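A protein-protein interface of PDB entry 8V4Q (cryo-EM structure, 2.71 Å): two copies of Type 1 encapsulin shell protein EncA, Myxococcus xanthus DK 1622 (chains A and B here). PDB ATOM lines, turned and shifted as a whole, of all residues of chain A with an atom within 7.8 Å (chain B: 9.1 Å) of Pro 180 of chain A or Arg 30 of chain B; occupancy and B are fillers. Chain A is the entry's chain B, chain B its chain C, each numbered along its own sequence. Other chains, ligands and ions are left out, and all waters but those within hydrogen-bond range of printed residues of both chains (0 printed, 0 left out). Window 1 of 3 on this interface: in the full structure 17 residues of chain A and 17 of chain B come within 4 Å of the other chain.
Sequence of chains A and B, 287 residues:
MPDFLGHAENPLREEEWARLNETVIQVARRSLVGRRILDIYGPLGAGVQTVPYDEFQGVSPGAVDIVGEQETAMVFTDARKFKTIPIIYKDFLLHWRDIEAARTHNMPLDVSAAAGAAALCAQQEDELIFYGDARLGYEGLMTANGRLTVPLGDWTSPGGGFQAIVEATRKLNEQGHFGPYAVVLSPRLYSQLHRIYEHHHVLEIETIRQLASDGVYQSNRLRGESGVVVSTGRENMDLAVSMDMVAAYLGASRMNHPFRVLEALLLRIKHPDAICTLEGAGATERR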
ATOM      1  N   ASP A  39      -0.067 -13.827   9.104  1.00  0.00           N
ATOM      2  CA  ASP A  39      -1.094 -13.614  10.111  1.00  0.00           C
ATOM      3  C   ASP A  39      -2.067 -12.529   9.656  1.00  0.00           C
ATOM      4  O   ASP A  39      -1.743 -11.674   8.828  1.00  0.00           O
ATOM      5  CB  ASP A  39      -0.468 -13.230  11.452  1.00  0.00           C
ATOM      6  CG  ASP A  39       0.038 -14.430  12.225  1.00  0.00           C
ATOM      7  OD1 ASP A  39      -0.730 -15.400  12.389  1.00  0.00           O
ATOM      8  OD2 ASP A  39       1.204 -14.404  12.670  1.00  0.00           O
ATOM      9  N   LEU A 172      19.814 -15.076   7.409  1.00  0.00           N
ATOM     10  CA  LEU A 172      18.688 -14.637   8.230  1.00  0.00           C
ATOM     11  C   LEU A 172      19.011 -14.753   9.715  1.00  0.00           C
ATOM     12  O   LEU A 172      18.651 -13.877  10.509  1.00  0.00           O
ATOM     13  CB  LEU A 172      17.438 -15.446   7.889  1.00  0.00           C
ATOM     14  CG  LEU A 172      16.573 -14.925   6.740  1.00  0.00           C
ATOM     15  CD1 LEU A 172      15.515 -15.947   6.354  1.00  0.00           C
ATOM     16  CD2 LEU A 172      15.932 -13.602   7.115  1.00  0.00           C
ATOM     17  N   HIS A 177      16.977 -13.248  13.497  1.00  0.00           N
ATOM     18  CA  HIS A 177      15.706 -13.857  13.119  1.00  0.00           C
ATOM     19  C   HIS A 177      15.924 -15.362  13.040  1.00  0.00           C
ATOM     20  O   HIS A 177      16.719 -15.838  12.223  1.00  0.00           O
ATOM     21  CB  HIS A 177      15.200 -13.284  11.797  1.00  0.00           C
ATOM     22  CG  HIS A 177      14.912 -11.816  11.854  1.00  0.00           C
ATOM     23  ND1 HIS A 177      13.782 -11.303  12.453  1.00  0.00           N
ATOM     24  CD2 HIS A 177      15.613 -10.751  11.401  1.00  0.00           C
ATOM     25  CE1 HIS A 177      13.797  -9.985  12.360  1.00  0.00           C
ATOM     26  NE2 HIS A 177      14.898  -9.625  11.725  1.00  0.00           N
ATOM     27  N   PHE A 178      15.215 -16.107  13.887  1.00  0.00           N
ATOM     28  CA  PHE A 178      15.533 -17.504  14.145  1.00  0.00           C
ATOM     29  C   PHE A 178      14.507 -18.483  13.594  1.00  0.00           C
ATOM     30  O   PHE A 178      14.711 -19.696  13.708  1.00  0.00           O
ATOM     31  CB  PHE A 178      15.690 -17.725  15.652  1.00  0.00           C
ATOM     32  CG  PHE A 178      16.557 -16.701  16.326  1.00  0.00           C
ATOM     33  CD1 PHE A 178      17.919 -16.661  16.084  1.00  0.00           C
ATOM     34  CD2 PHE A 178      16.011 -15.783  17.205  1.00  0.00           C
ATOM     35  CE1 PHE A 178      18.720 -15.722  16.702  1.00  0.00           C
ATOM     36  CE2 PHE A 178      16.808 -14.841  17.827  1.00  0.00           C
ATOM     37  CZ  PHE A 178      18.164 -14.811  17.575  1.00  0.00           C
ATOM     38  N   GLY A 179      13.415 -18.005  13.008  1.00  0.00           N
ATOM     39  CA  GLY A 179      12.427 -18.885  12.438  1.00  0.00           C
ATOM     40  C   GLY A 179      11.196 -19.037  13.309  1.00  0.00           C
ATOM     41  O   GLY A 179      11.014 -18.314  14.293  1.00  0.00           O
ATOM     42  N   PRO A 180      10.315 -19.989  12.963  1.00  0.00           N
ATOM     43  CA  PRO A 180      10.393 -20.942  11.837  1.00  0.00           C
ATOM     44  C   PRO A 180      10.284 -20.270  10.471  1.00  0.00           C
ATOM     45  O   PRO A 180       9.774 -19.160  10.353  1.00  0.00           O
ATOM     46  CB  PRO A 180       9.210 -21.888  12.101  1.00  0.00           C
ATOM     47  CG  PRO A 180       8.266 -21.106  12.963  1.00  0.00           C
ATOM     48  CD  PRO A 180       9.150 -20.257  13.823  1.00  0.00           C
ATOM     49  N   TYR A 181      10.766 -20.929   9.422  1.00  0.00           N
ATOM     50  CA  TYR A 181      10.911 -20.325   8.108  1.00  0.00           C
ATOM     51  C   TYR A 181       9.906 -20.912   7.127  1.00  0.00           C
ATOM     52  O   TYR A 181       9.514 -22.077   7.231  1.00  0.00           O
ATOM     53  CB  TYR A 181      12.327 -20.536   7.564  1.00  0.00           C
ATOM     54  CG  TYR A 181      13.427 -20.033   8.470  1.00  0.00           C
ATOM     55  CD1 TYR A 181      13.638 -18.674   8.651  1.00  0.00           C
ATOM     56  CD2 TYR A 181      14.259 -20.920   9.137  1.00  0.00           C
ATOM     57  CE1 TYR A 181      14.646 -18.213   9.477  1.00  0.00           C
ATOM     58  CE2 TYR A 181      15.267 -20.470   9.963  1.00  0.00           C
ATOM     59  CZ  TYR A 181      15.457 -19.116  10.130  1.00  0.00           C
ATOM     60  OH  TYR A 181      16.462 -18.667  10.953  1.00  0.00           O
ATOM     61  N   ALA A 182       9.499 -20.088   6.165  1.00  0.00           N
ATOM     62  CA  ALA A 182       8.653 -20.515   5.061  1.00  0.00           C
ATOM     63  C   ALA A 182       9.335 -20.174   3.744  1.00  0.00           C
ATOM     64  O   ALA A 182      10.039 -19.164   3.636  1.00  0.00           O
ATOM     65  CB  ALA A 182       7.271 -19.856   5.123  1.00  0.00           C
ATOM     66  N   LEU A 211      13.939 -28.284   6.833  1.00  0.00           N
ATOM     67  CA  LEU A 211      14.611 -27.032   7.165  1.00  0.00           C
ATOM     68  C   LEU A 211      13.673 -25.835   7.230  1.00  0.00           C
ATOM     69  O   LEU A 211      14.037 -24.817   7.830  1.00  0.00           O
ATOM     70  CB  LEU A 211      15.732 -26.733   6.161  1.00  0.00           C
ATOM     71  CG  LEU A 211      17.124 -27.258   6.526  1.00  0.00           C
ATOM     72  CD1 LEU A 211      17.182 -28.773   6.474  1.00  0.00           C
ATOM     73  CD2 LEU A 211      18.191 -26.645   5.625  1.00  0.00           C
ATOM     74  N   ALA A 212      12.489 -25.926   6.632  1.00  0.00           N
ATOM     75  CA  ALA A 212      11.462 -24.892   6.713  1.00  0.00           C
ATOM     76  C   ALA A 212      10.203 -25.552   7.267  1.00  0.00           C
ATOM     77  O   ALA A 212       9.425 -26.154   6.524  1.00  0.00           O
ATOM     78  CB  ALA A 212      11.215 -24.251   5.351  1.00  0.00           C
ATOM     79  N   SER A 213      10.003 -25.435   8.582  1.00  0.00           N
ATOM     80  CA  SER A 213       8.889 -26.119   9.226  1.00  0.00           C
ATOM     81  C   SER A 213       7.553 -25.421   9.006  1.00  0.00           C
ATOM     82  O   SER A 213       6.516 -25.994   9.356  1.00  0.00           O
ATOM     83  CB  SER A 213       9.155 -26.266  10.725  1.00  0.00           C
ATOM     84  OG  SER A 213       9.177 -25.009  11.372  1.00  0.00           O
ATOM     85  N   ASP A 214       7.545 -24.213   8.446  1.00  0.00           N
ATOM     86  CA  ASP A 214       6.298 -23.542   8.109  1.00  0.00           C
ATOM     87  C   ASP A 214       5.810 -23.858   6.702  1.00  0.00           C
ATOM     88  O   ASP A 214       4.690 -23.471   6.353  1.00  0.00           O
ATOM     89  CB  ASP A 214       6.445 -22.025   8.263  1.00  0.00           C
ATOM     90  CG  ASP A 214       6.260 -21.565   9.691  1.00  0.00           C
ATOM     91  OD1 ASP A 214       5.459 -22.188  10.419  1.00  0.00           O
ATOM     92  OD2 ASP A 214       6.910 -20.576  10.087  1.00  0.00           O
ATOM     93  N   GLY A 215       6.611 -24.541   5.893  1.00  0.00           N
ATOM     94  CA  GLY A 215       6.161 -25.000   4.592  1.00  0.00           C
ATOM     95  C   GLY A 215       6.957 -24.515   3.398  1.00  0.00           C
ATOM     96  O   GLY A 215       7.633 -23.482   3.443  1.00  0.00           O
ATOM     97  N   VAL A 229      12.527 -16.655   1.051  1.00  0.00           N
ATOM     98  CA  VAL A 229      12.532 -17.303   2.356  1.00  0.00           C
ATOM     99  C   VAL A 229      12.196 -16.245   3.396  1.00  0.00           C
ATOM    100  O   VAL A 229      12.850 -15.195   3.457  1.00  0.00           O
ATOM    101  CB  VAL A 229      13.890 -17.963   2.660  1.00  0.00           C
ATOM    102  CG1 VAL A 229      13.839 -18.705   3.986  1.00  0.00           C
ATOM    103  CG2 VAL A 229      14.290 -18.900   1.534  1.00  0.00           C
ATOM    104  N   VAL A 230      11.177 -16.516   4.208  1.00  0.00           N
ATOM    105  CA  VAL A 230      10.689 -15.554   5.187  1.00  0.00           C
ATOM    106  C   VAL A 230      10.703 -16.185   6.571  1.00  0.00           C
ATOM    107  O   VAL A 230      10.334 -17.353   6.741  1.00  0.00           O
ATOM    108  CB  VAL A 230       9.276 -15.037   4.838  1.00  0.00           C
ATOM    109  CG1 VAL A 230       9.322 -14.168   3.593  1.00  0.00           C
ATOM    110  CG2 VAL A 230       8.310 -16.194   4.645  1.00  0.00           C
ATOM    111  N   SER A 231      11.148 -15.409   7.557  1.00  0.00           N
ATOM    112  CA  SER A 231      11.049 -15.783   8.963  1.00  0.00           C
ATOM    113  C   SER A 231       9.694 -15.308   9.474  1.00  0.00           C
ATOM    114  O   SER A 231       9.490 -14.109   9.689  1.00  0.00           O
ATOM    115  CB  SER A 231      12.194 -15.174   9.767  1.00  0.00           C
ATOM    116  OG  SER A 231      12.047 -15.437  11.150  1.00  0.00           O
ATOM    117  N   THR A 232       8.770 -16.245   9.664  1.00  0.00           N
ATOM    118  CA  THR A 232       7.398 -15.887   9.991  1.00  0.00           C
ATOM    119  C   THR A 232       7.295 -15.357  11.415  1.00  0.00           C
ATOM    120  O   THR A 232       8.113 -15.670  12.284  1.00  0.00           O
ATOM    121  CB  THR A 232       6.474 -17.093   9.813  1.00  0.00           C
ATOM    122  OG1 THR A 232       6.743 -18.059  10.838  1.00  0.00           O
ATOM    123  CG2 THR A 232       6.692 -17.732   8.451  1.00  0.00           C
ATOM    124  N   GLY A 233       6.271 -14.540  11.646  1.00  0.00           N
ATOM    125  CA  GLY A 233       6.062 -13.918  12.938  1.00  0.00           C
ATOM    126  C   GLY A 233       5.170 -12.699  12.851  1.00  0.00           C
ATOM    127  O   GLY A 233       5.280 -11.908  11.910  1.00  0.00           O
ATOM    128  N   ARG A 234       4.280 -12.536  13.832  1.00  0.00           N
ATOM    129  CA  ARG A 234       3.334 -11.425  13.805  1.00  0.00           C
ATOM    130  C   ARG A 234       4.035 -10.080  13.954  1.00  0.00           C
ATOM    131  O   ARG A 234       3.556  -9.070  13.428  1.00  0.00           O
ATOM    132  CB  ARG A 234       2.287 -11.610  14.903  1.00  0.00           C
ATOM    133  CG  ARG A 234       1.144 -10.617  14.861  1.00  0.00           C
ATOM    134  CD  ARG A 234       0.169 -10.857  16.000  1.00  0.00           C
ATOM    135  NE  ARG A 234      -0.519 -12.136  15.876  1.00  0.00           N
ATOM    136  CZ  ARG A 234      -1.611 -12.332  15.148  1.00  0.00           C
ATOM    137  NH1 ARG A 234      -2.164 -11.353  14.453  1.00  0.00           N
ATOM    138  NH2 ARG A 234      -2.160 -13.543  15.117  1.00  0.00           N
ATOM    139  N   ASN A 236       6.953  -9.341  12.696  1.00  0.00           N
ATOM    140  CA  ASN A 236       7.733  -9.065  11.496  1.00  0.00           C
ATOM    141  C   ASN A 236       6.876  -8.618  10.321  1.00  0.00           C
ATOM    142  O   ASN A 236       7.285  -7.732   9.565  1.00  0.00           O
ATOM    143  CB  ASN A 236       8.539 -10.303  11.090  1.00  0.00           C
ATOM    144  CG  ASN A 236       9.633 -10.641  12.083  1.00  0.00           C
ATOM    145  OD1 ASN A 236      10.359  -9.763  12.546  1.00  0.00           O
ATOM    146  ND2 ASN A 236       9.760 -11.920  12.409  1.00  0.00           N
ATOM    147  N   THR B  23      -2.467 -15.445  22.994  1.00  0.00           N
ATOM    148  CA  THR B  23      -1.402 -15.105  22.059  1.00  0.00           C
ATOM    149  C   THR B  23      -0.032 -15.330  22.684  1.00  0.00           C
ATOM    150  O   THR B  23       0.872 -15.875  22.038  1.00  0.00           O
ATOM    151  CB  THR B  23      -1.548 -13.654  21.601  1.00  0.00           C
ATOM    152  OG1 THR B  23      -2.899 -13.414  21.190  1.00  0.00           O
ATOM    153  CG2 THR B  23      -0.608 -13.361  20.440  1.00  0.00           C
ATOM    154  N   VAL B  24       0.137 -14.923  23.945  1.00  0.00           N
ATOM    155  CA  VAL B  24       1.417 -15.119  24.624  1.00  0.00           C
ATOM    156  C   VAL B  24       1.745 -16.605  24.720  1.00  0.00           C
ATOM    157  O   VAL B  24       2.869 -17.034  24.420  1.00  0.00           O
ATOM    158  CB  VAL B  24       1.393 -14.454  26.012  1.00  0.00           C
ATOM    159  CG1 VAL B  24       2.531 -14.976  26.877  1.00  0.00           C
ATOM    160  CG2 VAL B  24       1.474 -12.942  25.877  1.00  0.00           C
ATOM    161  N   ILE B  25       0.764 -17.414  25.127  1.00  0.00           N
ATOM    162  CA  ILE B  25       0.994 -18.851  25.273  1.00  0.00           C
ATOM    163  C   ILE B  25       1.323 -19.482  23.924  1.00  0.00           C
ATOM    164  O   ILE B  25       2.254 -20.291  23.806  1.00  0.00           O
ATOM    165  CB  ILE B  25      -0.224 -19.526  25.930  1.00  0.00           C
ATOM    166  CG1 ILE B  25      -0.406 -19.018  27.360  1.00  0.00           C
ATOM    167  CG2 ILE B  25      -0.070 -21.037  25.920  1.00  0.00           C
ATOM    168  CD1 ILE B  25       0.768 -19.316  28.266  1.00  0.00           C
ATOM    169  N   GLN B  26       0.569 -19.117  22.883  1.00  0.00           N
ATOM    170  CA  GLN B  26       0.788 -19.688  21.560  1.00  0.00           C
ATOM    171  C   GLN B  26       2.165 -19.326  21.018  1.00  0.00           C
ATOM    172  O   GLN B  26       2.836 -20.162  20.402  1.00  0.00           O
ATOM    173  CB  GLN B  26      -0.309 -19.218  20.607  1.00  0.00           C
ATOM    174  CG  GLN B  26      -0.173 -19.729  19.185  1.00  0.00           C
ATOM    175  CD  GLN B  26      -1.303 -19.258  18.290  1.00  0.00           C
ATOM    176  OE1 GLN B  26      -2.210 -18.554  18.734  1.00  0.00           O
ATOM    177  NE2 GLN B  26      -1.253 -19.643  17.020  1.00  0.00           N
ATOM    178  N   VAL B  27       2.602 -18.083  21.230  1.00  0.00           N
ATOM    179  CA  VAL B  27       3.923 -17.680  20.757  1.00  0.00           C
ATOM    180  C   VAL B  27       5.014 -18.411  21.530  1.00  0.00           C
ATOM    181  O   VAL B  27       6.006 -18.865  20.946  1.00  0.00           O
ATOM    182  CB  VAL B  27       4.081 -16.151  20.850  1.00  0.00           C
ATOM    183  CG1 VAL B  27       5.535 -15.752  20.665  1.00  0.00           C
ATOM    184  CG2 VAL B  27       3.207 -15.470  19.812  1.00  0.00           C
ATOM    185  N   ALA B  28       4.849 -18.549  22.848  1.00  0.00           N
ATOM    186  CA  ALA B  28       5.864 -19.237  23.641  1.00  0.00           C
ATOM    187  C   ALA B  28       5.939 -20.722  23.309  1.00  0.00           C
ATOM    188  O   ALA B  28       7.002 -21.335  23.458  1.00  0.00           O
ATOM    189  CB  ALA B  28       5.590 -19.045  25.130  1.00  0.00           C
ATOM    190  N   ARG B  29       4.830 -21.317  22.861  1.00  0.00           N
ATOM    191  CA  ARG B  29       4.803 -22.760  22.637  1.00  0.00           C
ATOM    192  C   ARG B  29       5.715 -23.179  21.488  1.00  0.00           C
ATOM    193  O   ARG B  29       6.354 -24.236  21.553  1.00  0.00           O
ATOM    194  CB  ARG B  29       3.372 -23.222  22.369  1.00  0.00           C
ATOM    195  CG  ARG B  29       3.055 -24.596  22.930  1.00  0.00           C
ATOM    196  CD  ARG B  29       1.750 -25.137  22.364  1.00  0.00           C
ATOM    197  NE  ARG B  29       0.570 -24.570  23.007  1.00  0.00           N
ATOM    198  CZ  ARG B  29       0.234 -24.756  24.277  1.00  0.00           C
ATOM    199  NH1 ARG B  29       0.958 -25.516  25.083  1.00  0.00           N
ATOM    200  NH2 ARG B  29      -0.864 -24.172  24.748  1.00  0.00           N
ATOM    201  N   ARG B  30       5.789 -22.376  20.430  1.00  0.00           N
ATOM    202  CA  ARG B  30       6.416 -22.802  19.184  1.00  0.00           C
ATOM    203  C   ARG B  30       7.879 -22.395  19.057  1.00  0.00           C
ATOM    204  O   ARG B  30       8.453 -22.559  17.975  1.00  0.00           O
ATOM    205  CB  ARG B  30       5.633 -22.251  17.988  1.00  0.00           C
ATOM    206  CG  ARG B  30       5.693 -20.740  17.848  1.00  0.00           C
ATOM    207  CD  ARG B  30       4.744 -20.247  16.769  1.00  0.00           C
ATOM    208  NE  ARG B  30       5.144 -20.702  15.443  1.00  0.00           N
ATOM    209  CZ  ARG B  30       4.370 -20.652  14.368  1.00  0.00           C
ATOM    210  NH1 ARG B  30       3.140 -20.168  14.424  1.00  0.00           N
ATOM    211  NH2 ARG B  30       4.842 -21.097  13.206  1.00  0.00           N
ATOM    212  N   SER B  31       8.501 -21.874  20.115  1.00  0.00           N
ATOM    213  CA  SER B  31       9.887 -21.426  20.031  1.00  0.00           C
ATOM    214  C   SER B  31      10.708 -21.894  21.227  1.00  0.00           C
ATOM    215  O   SER B  31      11.725 -21.282  21.564  1.00  0.00           O
ATOM    216  CB  SER B  31       9.959 -19.906  19.896  1.00  0.00           C
ATOM    217  OG  SER B  31       9.681 -19.269  21.129  1.00  0.00           O
ATOM    218  N   LEU B  32      10.289 -22.977  21.876  1.00  0.00           N
ATOM    219  CA  LEU B  32      10.996 -23.526  23.025  1.00  0.00           C
ATOM    220  C   LEU B  32      11.504 -24.921  22.691  1.00  0.00           C
ATOM    221  O   LEU B  32      10.743 -25.764  22.205  1.00  0.00           O
ATOM    222  CB  LEU B  32      10.093 -23.570  24.261  1.00  0.00           C
ATOM    223  CG  LEU B  32       9.921 -22.244  25.004  1.00  0.00           C
ATOM    224  CD1 LEU B  32       8.864 -22.366  26.091  1.00  0.00           C
ATOM    225  CD2 LEU B  32      11.245 -21.772  25.585  1.00  0.00           C
ATOM    226  N   VAL B  33      12.788 -25.159  22.954  1.00  0.00           N
ATOM    227  CA  VAL B  33      13.400 -26.450  22.691  1.00  0.00           C
ATOM    228  C   VAL B  33      13.781 -27.186  23.974  1.00  0.00           C
ATOM    229  O   VAL B  33      13.720 -28.420  24.007  1.00  0.00           O
ATOM    230  CB  VAL B  33      14.628 -26.278  21.770  1.00  0.00           C
ATOM    231  CG1 VAL B  33      15.440 -27.563  21.673  1.00  0.00           C
ATOM    232  CG2 VAL B  33      14.193 -25.814  20.389  1.00  0.00           C
ATOM    233  N   ARG B  36      11.160 -29.653  25.568  1.00  0.00           N
ATOM    234  CA  ARG B  36      10.864 -30.884  24.778  1.00  0.00           C
ATOM    235  C   ARG B  36      11.765 -32.061  25.162  1.00  0.00           C
ATOM    236  O   ARG B  36      11.537 -33.141  24.663  1.00  0.00           O
ATOM    237  CB  ARG B  36      11.162 -30.629  23.303  1.00  0.00           C
ATOM    238  CG  ARG B  36       9.971 -30.191  22.469  1.00  0.00           C
ATOM    239  CD  ARG B  36      10.387 -30.007  21.028  1.00  0.00           C
ATOM    240  NE  ARG B  36      10.476 -28.594  20.706  1.00  0.00           N
ATOM    241  CZ  ARG B  36      10.625 -28.096  19.484  1.00  0.00           C
ATOM    242  NH1 ARG B  36      10.715 -28.904  18.443  1.00  0.00           N
ATOM    243  NH2 ARG B  36      10.682 -26.787  19.307  1.00  0.00           N
ATOM    244  N   ALA B 115       3.531 -10.523  21.365  1.00  0.00           N
ATOM    245  CA  ALA B 115       4.182 -11.631  20.675  1.00  0.00           C
ATOM    246  C   ALA B 115       5.694 -11.437  20.613  1.00  0.00           C
ATOM    247  O   ALA B 115       6.460 -12.385  20.836  1.00  0.00           O
ATOM    248  CB  ALA B 115       3.601 -11.785  19.270  1.00  0.00           C
ATOM    249  N   ALA B 118       7.106 -12.086  24.084  1.00  0.00           N
ATOM    250  CA  ALA B 118       7.102 -13.513  24.387  1.00  0.00           C
ATOM    251  C   ALA B 118       8.221 -14.243  23.653  1.00  0.00           C
ATOM    252  O   ALA B 118       8.859 -15.139  24.219  1.00  0.00           O
ATOM    253  CB  ALA B 118       5.743 -14.119  24.038  1.00  0.00           C
ATOM    254  N   ALA B 119       8.470 -13.881  22.391  1.00  0.00           N
ATOM    255  CA  ALA B 119       9.569 -14.501  21.657  1.00  0.00           C
ATOM    256  C   ALA B 119      10.912 -14.198  22.314  1.00  0.00           C
ATOM    257  O   ALA B 119      11.765 -15.089  22.452  1.00  0.00           O
ATOM    258  CB  ALA B 119       9.562 -14.029  20.205  1.00  0.00           C
ATOM    259  N   ALA B 122      11.230 -16.299  25.455  1.00  0.00           N
ATOM    260  CA  ALA B 122      11.558 -17.685  25.136  1.00  0.00           C
ATOM    261  C   ALA B 122      13.032 -17.834  24.777  1.00  0.00           C
ATOM    262  O   ALA B 122      13.686 -18.805  25.182  1.00  0.00           O
ATOM    263  CB  ALA B 122      10.673 -18.185  23.998  1.00  0.00           C
ATOM    264  N   GLN B 123      13.572 -16.881  24.010  1.00  0.00           N
ATOM    265  CA  GLN B 123      14.999 -16.911  23.703  1.00  0.00           C
ATOM    266  C   GLN B 123      15.838 -16.832  24.974  1.00  0.00           C
ATOM    267  O   GLN B 123      16.824 -17.568  25.129  1.00  0.00           O
ATOM    268  CB  GLN B 123      15.355 -15.768  22.754  1.00  0.00           C
ATOM    269  CG  GLN B 123      15.093 -16.065  21.287  1.00  0.00           C
ATOM    270  CD  GLN B 123      16.001 -17.147  20.737  1.00  0.00           C
ATOM    271  OE1 GLN B 123      17.195 -16.929  20.542  1.00  0.00           O
ATOM    272  NE2 GLN B 123      15.436 -18.321  20.482  1.00  0.00           N
ATOM    273  N   ASP B 126      15.703 -20.218  26.827  1.00  0.00           N
ATOM    274  CA  ASP B 126      16.562 -21.222  26.204  1.00  0.00           C
ATOM    275  C   ASP B 126      18.033 -20.947  26.491  1.00  0.00           C
ATOM    276  O   ASP B 126      18.809 -21.877  26.755  1.00  0.00           O
ATOM    277  CB  ASP B 126      16.310 -21.276  24.697  1.00  0.00           C
ATOM    278  CG  ASP B 126      15.140 -22.168  24.334  1.00  0.00           C
ATOM    279  OD1 ASP B 126      14.865 -23.127  25.086  1.00  0.00           O
ATOM    280  OD2 ASP B 126      14.496 -21.915  23.294  1.00  0.00           O
ATOM    281  N   GLN B 218      17.537 -29.163  16.786  1.00  0.00           N
ATOM    282  CA  GLN B 218      18.484 -28.088  16.522  1.00  0.00           C
ATOM    283  C   GLN B 218      18.191 -26.928  17.462  1.00  0.00           C
ATOM    284  O   GLN B 218      17.026 -26.638  17.754  1.00  0.00           O
ATOM    285  CB  GLN B 218      18.422 -27.618  15.065  1.00  0.00           C
ATOM    286  CG  GLN B 218      17.104 -26.980  14.657  1.00  0.00           C
ATOM    287  CD  GLN B 218      17.108 -26.499  13.219  1.00  0.00           C
ATOM    288  OE1 GLN B 218      18.127 -26.569  12.533  1.00  0.00           O
ATOM    289  NE2 GLN B 218      15.964 -26.011  12.755  1.00  0.00           N
ATOM    290  N   ASN B 220      19.465 -22.809  18.238  1.00  0.00           N
ATOM    291  CA  ASN B 220      20.230 -21.648  17.805  1.00  0.00           C
ATOM    292  C   ASN B 220      21.105 -21.062  18.904  1.00  0.00           C
ATOM    293  O   ASN B 220      22.030 -20.303  18.595  1.00  0.00           O
ATOM    294  CB  ASN B 220      19.285 -20.571  17.271  1.00  0.00           C
ATOM    295  CG  ASN B 220      18.269 -20.121  18.303  1.00  0.00           C
ATOM    296  OD1 ASN B 220      18.305 -20.545  19.457  1.00  0.00           O
ATOM    297  ND2 ASN B 220      17.355 -19.259  17.892  1.00  0.00           N
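The guanidinium group of Arg 30 of chain B lies within salt-bridge range of the side-chain carboxylate of Asp 214 of chain A, 3.1 Å away.
The backbone carbonyl oxygen (O) of Pro 180 of chain A is in hydrogen-bond range of the backbone NH (N) of Thr 232 of chain A (3.2 Å). The side-chain hydroxyl (OH) of Tyr 181 of chain A sits close to the backbone carbonyl oxygen (O) of Phe 178 of chain A (3.4 Å). ND2 of Asn 220 of chain B sits close to NE2 of Gln 123 of chain B (3.4 Å). O of Tyr 181 of chain A lies within hydrogen-bond range of N of Asp 214 of chain A (3.1 Å). OG1 of Thr 232 of chain A lies within hydrogen-bond range of OD2 of Asp 214 of chain A (2.6 Å).
Gln 123 of chain B touches Phe 178 of chain A. Phe 178 of chain A touches Asn 220 of chain B. Pro 180 of chain A touches Arg 30 of chain B.
Printed residues of chain A within 4 Å of Arg 30 of chain B: Pro 180 and Asp 214. No residue of chain B comes within 4 Å of Gly 179 of chain A. No residue of chain B comes within 4 Å of Thr 232 of chain A. Of the printed residues of chain A, Gln 123 of chain B touches Phe 178 (3.4 Å). Printed residues of chain B within 4 Å of Phe 178 of chain A: Gln 123 (3.4 Å) and Asn 220 (3.1 Å). Printed residues of chain A within 4 Å of Asn 220 of chain B: Phe 178. Printed residues of chain B within 4 Å of Asp 214 of chain A: Arg 30 (3.1 Å). Asn 236 of chain A touches none of the printed residues of chain B. The nearest residue of chain A that does not touch Arg 30 of chain B is Thr 232 of chain A (4.3 Å). The nearest printed residue of chain A that does not touch Gln 123 of chain B is Gly 179 of chain A (7.6 Å).
Hydrophobic or aromatic side chains of chain A that line the printed part of chain B: Phe 178 and Pro 180. Among the printed residues, 4 pairs touch across the chains.
No position is printed for both chains. Of the 4 pairs that touch across the chains among the printed residues, none has its exchanged pair printed and touching as well.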
